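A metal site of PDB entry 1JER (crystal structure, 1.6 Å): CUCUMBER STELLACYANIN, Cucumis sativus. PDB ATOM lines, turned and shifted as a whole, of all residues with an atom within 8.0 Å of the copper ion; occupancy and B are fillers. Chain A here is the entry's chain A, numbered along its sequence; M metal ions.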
ATOM      1  N   TRP A  14     -26.648   5.558  11.480  1.00  0.00           N
ATOM      2  CA  TRP A  14     -26.221   6.630  10.578  1.00  0.00           C
ATOM      3  C   TRP A  14     -27.450   7.119   9.787  1.00  0.00           C
ATOM      4  O   TRP A  14     -27.971   6.360   8.975  1.00  0.00           O
ATOM      5  CB  TRP A  14     -25.245   5.983   9.589  1.00  0.00           C
ATOM      6  CG  TRP A  14     -24.508   6.865   8.637  1.00  0.00           C
ATOM      7  CD1 TRP A  14     -24.425   6.589   7.270  1.00  0.00           C
ATOM      8  CD2 TRP A  14     -23.725   8.033   8.844  1.00  0.00           C
ATOM      9  NE1 TRP A  14     -23.657   7.556   6.664  1.00  0.00           N
ATOM     10  CE2 TRP A  14     -23.215   8.460   7.589  1.00  0.00           C
ATOM     11  CE3 TRP A  14     -23.426   8.826   9.965  1.00  0.00           C
ATOM     12  CZ2 TRP A  14     -22.422   9.573   7.399  1.00  0.00           C
ATOM     13  CZ3 TRP A  14     -22.617   9.957   9.771  1.00  0.00           C
ATOM     14  CH2 TRP A  14     -22.112  10.325   8.524  1.00  0.00           C
ATOM     15  N   SER A  15     -27.934   8.306  10.105  1.00  0.00           N
ATOM     16  CA  SER A  15     -29.124   8.796   9.346  1.00  0.00           C
ATOM     17  C   SER A  15     -29.098  10.302   9.406  1.00  0.00           C
ATOM     18  O   SER A  15     -28.168  10.900   9.996  1.00  0.00           O
ATOM     19  CB  SER A  15     -30.416   8.213   9.866  1.00  0.00           C
ATOM     20  OG  SER A  15     -30.675   8.544  11.211  1.00  0.00           O
ATOM     21  N   VAL A  16     -30.065  10.976   8.812  1.00  0.00           N
ATOM     22  CA  VAL A  16     -30.069  12.446   8.959  1.00  0.00           C
ATOM     23  C   VAL A  16     -30.663  12.772  10.323  1.00  0.00           C
ATOM     24  O   VAL A  16     -31.788  12.398  10.633  1.00  0.00           O
ATOM     25  CB  VAL A  16     -31.018  13.039   7.864  1.00  0.00           C
ATOM     26  CG1 VAL A  16     -31.075  14.538   8.028  1.00  0.00           C
ATOM     27  CG2 VAL A  16     -30.416  12.663   6.505  1.00  0.00           C
ATOM     28  N   PHE A  42     -27.252   1.526   8.475  1.00  0.00           N
ATOM     29  CA  PHE A  42     -28.373   2.373   7.928  1.00  0.00           C
ATOM     30  C   PHE A  42     -29.175   1.444   7.005  1.00  0.00           C
ATOM     31  O   PHE A  42     -28.680   0.411   6.559  1.00  0.00           O
ATOM     32  CB  PHE A  42     -27.771   3.494   7.142  1.00  0.00           C
ATOM     33  CG  PHE A  42     -26.695   3.162   6.152  1.00  0.00           C
ATOM     34  CD1 PHE A  42     -25.362   3.074   6.550  1.00  0.00           C
ATOM     35  CD2 PHE A  42     -27.004   2.938   4.810  1.00  0.00           C
ATOM     36  CE1 PHE A  42     -24.377   2.778   5.609  1.00  0.00           C
ATOM     37  CE2 PHE A  42     -26.032   2.645   3.885  1.00  0.00           C
ATOM     38  CZ  PHE A  42     -24.693   2.546   4.277  1.00  0.00           C
ATOM     39  N   ASN A  45     -29.404   1.266   0.561  1.00  0.00           N
ATOM     40  CA  ASN A  45     -29.888   2.159  -0.447  1.00  0.00           C
ATOM     41  C   ASN A  45     -30.327   3.517  -0.027  1.00  0.00           C
ATOM     42  O   ASN A  45     -30.517   4.377  -0.922  1.00  0.00           O
ATOM     43  CB  ASN A  45     -30.958   1.457  -1.309  1.00  0.00           C
ATOM     44  CG  ASN A  45     -30.378   0.555  -2.377  1.00  0.00           C
ATOM     45  OD1 ASN A  45     -29.283  -0.003  -2.251  1.00  0.00           O
ATOM     46  ND2 ASN A  45     -31.106   0.384  -3.482  1.00  0.00           N
ATOM     47  N   ALA A  46     -30.478   3.840   1.264  1.00  0.00           N
ATOM     48  CA  ALA A  46     -30.922   5.167   1.675  1.00  0.00           C
ATOM     49  C   ALA A  46     -29.778   6.151   1.911  1.00  0.00           C
ATOM     50  O   ALA A  46     -29.935   7.363   1.836  1.00  0.00           O
ATOM     51  CB  ALA A  46     -31.713   5.059   2.987  1.00  0.00           C
ATOM     52  N   HIS A  47     -28.608   5.633   2.296  1.00  0.00           N
ATOM     53  CA  HIS A  47     -27.483   6.612   2.557  1.00  0.00           C
ATOM     54  C   HIS A  47     -26.217   5.950   2.038  1.00  0.00           C
ATOM     55  O   HIS A  47     -26.211   4.843   1.515  1.00  0.00           O
ATOM     56  CB  HIS A  47     -27.335   6.642   4.150  1.00  0.00           C
ATOM     57  CG  HIS A  47     -28.546   7.243   4.779  1.00  0.00           C
ATOM     58  ND1 HIS A  47     -28.845   8.574   4.655  1.00  0.00           N
ATOM     59  CD2 HIS A  47     -29.567   6.670   5.488  1.00  0.00           C
ATOM     60  CE1 HIS A  47     -29.994   8.827   5.305  1.00  0.00           C
ATOM     61  NE2 HIS A  47     -30.440   7.693   5.815  1.00  0.00           N
ATOM     62  N   ASN A  48     -25.079   6.612   2.286  1.00  0.00           N
ATOM     63  CA  ASN A  48     -23.805   5.966   1.965  1.00  0.00           C
ATOM     64  C   ASN A  48     -22.770   6.564   2.937  1.00  0.00           C
ATOM     65  O   ASN A  48     -23.168   7.362   3.810  1.00  0.00           O
ATOM     66  CB  ASN A  48     -23.398   6.155   0.522  1.00  0.00           C
ATOM     67  CG  ASN A  48     -23.306   7.609   0.100  1.00  0.00           C
ATOM     68  OD1 ASN A  48     -23.583   7.944  -1.064  1.00  0.00           O
ATOM     69  ND2 ASN A  48     -23.000   8.473   1.004  1.00  0.00           N
ATOM     70  N   VAL A  49     -21.533   6.110   2.804  1.00  0.00           N
ATOM     71  CA  VAL A  49     -20.464   6.618   3.654  1.00  0.00           C
ATOM     72  C   VAL A  49     -19.250   6.915   2.770  1.00  0.00           C
ATOM     73  O   VAL A  49     -18.793   6.033   2.065  1.00  0.00           O
ATOM     74  CB  VAL A  49     -20.019   5.548   4.682  1.00  0.00           C
ATOM     75  CG1 VAL A  49     -18.921   6.229   5.557  1.00  0.00           C
ATOM     76  CG2 VAL A  49     -21.198   5.169   5.587  1.00  0.00           C
ATOM     77  N   ARG A  72     -24.208   1.233  -1.572  1.00  0.00           N
ATOM     78  CA  ARG A  72     -25.110   1.700  -0.512  1.00  0.00           C
ATOM     79  C   ARG A  72     -25.489   0.543   0.395  1.00  0.00           C
ATOM     80  O   ARG A  72     -26.563   0.514   0.971  1.00  0.00           O
ATOM     81  CB  ARG A  72     -26.365   2.307  -1.128  1.00  0.00           C
ATOM     82  CG  ARG A  72     -26.092   3.604  -1.903  1.00  0.00           C
ATOM     83  CD  ARG A  72     -27.215   4.635  -1.777  1.00  0.00           C
ATOM     84  NE  ARG A  72     -27.090   5.739  -2.733  1.00  0.00           N
ATOM     85  CZ  ARG A  72     -28.125   6.472  -3.161  1.00  0.00           C
ATOM     86  NH1 ARG A  72     -29.366   6.228  -2.725  1.00  0.00           N
ATOM     87  NH2 ARG A  72     -28.022   7.490  -4.025  1.00  0.00           N
ATOM     88  N   VAL A  89     -18.872  11.541   5.362  1.00  0.00           N
ATOM     89  CA  VAL A  89     -20.190  12.187   5.129  1.00  0.00           C
ATOM     90  C   VAL A  89     -21.058  11.173   4.354  1.00  0.00           C
ATOM     91  O   VAL A  89     -20.578  10.184   3.846  1.00  0.00           O
ATOM     92  CB  VAL A  89     -20.013  13.412   4.201  1.00  0.00           C
ATOM     93  CG1 VAL A  89     -19.130  14.462   4.877  1.00  0.00           C
ATOM     94  CG2 VAL A  89     -19.360  12.986   2.893  1.00  0.00           C
ATOM     95  N   CYS A  90     -22.318  11.550   4.277  1.00  0.00           N
ATOM     96  CA  CYS A  90     -23.236  10.847   3.369  1.00  0.00           C
ATOM     97  C   CYS A  90     -23.425  11.807   2.166  1.00  0.00           C
ATOM     98  O   CYS A  90     -23.639  13.004   2.386  1.00  0.00           O
ATOM     99  CB  CYS A  90     -24.628  10.736   4.071  1.00  0.00           C
ATOM    100  SG  CYS A  90     -25.800   9.965   2.857  1.00  0.00           S
ATOM    101  N   THR A  91     -23.237  11.299   0.959  1.00  0.00           N
ATOM    102  CA  THR A  91     -23.262  12.175  -0.224  1.00  0.00           C
ATOM    103  C   THR A  91     -24.615  12.155  -0.900  1.00  0.00           C
ATOM    104  O   THR A  91     -24.791  12.726  -1.970  1.00  0.00           O
ATOM    105  CB  THR A  91     -22.179  11.807  -1.239  1.00  0.00           C
ATOM    106  OG1 THR A  91     -22.402  10.519  -1.777  1.00  0.00           O
ATOM    107  CG2 THR A  91     -20.783  11.788  -0.599  1.00  0.00           C
ATOM    108  N   VAL A  92     -25.606  11.528  -0.260  1.00  0.00           N
ATOM    109  CA  VAL A  92     -26.961  11.534  -0.903  1.00  0.00           C
ATOM    110  C   VAL A  92     -27.612  12.863  -0.698  1.00  0.00           C
ATOM    111  O   VAL A  92     -27.725  13.379   0.399  1.00  0.00           O
ATOM    112  CB  VAL A  92     -27.805  10.410  -0.311  1.00  0.00           C
ATOM    113  CG1 VAL A  92     -29.279  10.547  -0.663  1.00  0.00           C
ATOM    114  CG2 VAL A  92     -27.257   9.043  -0.643  1.00  0.00           C
ATOM    115  N   GLY A  93     -28.149  13.443  -1.812  1.00  0.00           N
ATOM    116  CA  GLY A  93     -28.953  14.627  -1.670  1.00  0.00           C
ATOM    117  C   GLY A  93     -28.481  15.705  -0.785  1.00  0.00           C
ATOM    118  O   GLY A  93     -27.352  16.230  -0.955  1.00  0.00           O
ATOM    119  N   THR A  94     -29.304  16.159   0.160  1.00  0.00           N
ATOM    120  CA  THR A  94     -28.865  17.244   1.070  1.00  0.00           C
ATOM    121  C   THR A  94     -28.476  16.702   2.434  1.00  0.00           C
ATOM    122  O   THR A  94     -28.415  17.460   3.423  1.00  0.00           O
ATOM    123  CB  THR A  94     -30.055  18.231   1.282  1.00  0.00           C
ATOM    124  OG1 THR A  94     -31.171  17.482   1.745  1.00  0.00           O
ATOM    125  CG2 THR A  94     -30.488  18.784  -0.106  1.00  0.00           C
ATOM    126  N   HIS A  95     -28.266  15.400   2.557  1.00  0.00           N
ATOM    127  CA  HIS A  95     -28.021  14.818   3.892  1.00  0.00           C
ATOM    128  C   HIS A  95     -26.826  15.444   4.584  1.00  0.00           C
ATOM    129  O   HIS A  95     -26.832  15.731   5.790  1.00  0.00           O
ATOM    130  CB  HIS A  95     -27.828  13.307   3.735  1.00  0.00           C
ATOM    131  CG  HIS A  95     -29.053  12.628   3.226  1.00  0.00           C
ATOM    132  ND1 HIS A  95     -29.149  11.269   3.156  1.00  0.00           N
ATOM    133  CD2 HIS A  95     -30.228  13.115   2.752  1.00  0.00           C
ATOM    134  CE1 HIS A  95     -30.328  10.895   2.683  1.00  0.00           C
ATOM    135  NE2 HIS A  95     -31.001  12.021   2.421  1.00  0.00           N
ATOM    136  N   CYS A  96     -25.729  15.659   3.831  1.00  0.00           N
ATOM    137  CA  CYS A  96     -24.552  16.247   4.529  1.00  0.00           C
ATOM    138  C   CYS A  96     -24.883  17.622   5.007  1.00  0.00           C
ATOM    139  O   CYS A  96     -24.626  18.017   6.154  1.00  0.00           O
ATOM    140  CB  CYS A  96     -23.393  16.228   3.526  1.00  0.00           C
ATOM    141  SG  CYS A  96     -21.867  17.005   4.073  1.00  0.00           S
ATOM    142  N   GLN A 100     -25.624  15.094   8.388  1.00  0.00           N
ATOM    143  CA  GLN A 100     -25.168  13.698   8.365  1.00  0.00           C
ATOM    144  C   GLN A 100     -23.690  13.704   7.923  1.00  0.00           C
ATOM    145  O   GLN A 100     -23.355  13.415   6.786  1.00  0.00           O
ATOM    146  CB  GLN A 100     -25.968  12.798   7.438  1.00  0.00           C
ATOM    147  CG  GLN A 100     -25.674  11.329   7.587  1.00  0.00           C
ATOM    148  CD  GLN A 100     -26.557  10.430   6.749  1.00  0.00           C
ATOM    149  OE1 GLN A 100     -27.198  10.890   5.799  1.00  0.00           O
ATOM    150  NE2 GLN A 100     -26.634   9.167   7.103  1.00  0.00           N
HETATM  151 CU    CU M   1     -27.734   9.978   3.853  1.00  0.00          CU
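The backbone NH (N) of Ser 15 sits close to the side-chain amide nitrogen (NE2) of Gln 100 (3.4 Å).
SG of Cys 90 lies close to N of Asn 48 (3.5 Å).
NE2 of Gln 100 sits close to NE1 of Trp 14 (3.4 Å).
The side-chain sulfur (SG) of Cys 90 lies close to the backbone NH (N) of Val 92 (3.5 Å).
O of Ala 46 touches the copper ion, at 3.97 Å.
Of the 19 residues printed, 5 come within 4 Å of the copper ion.
The copper ion is bound by ND1 of His 47 (2.0 Å).
ND1 of His 95 binds the copper ion (2.0 Å).
SG of Cys 90 binds the copper ion (2.2 Å).
The copper ion is bound by the side-chain amide oxygen (OE1) of Gln 100.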
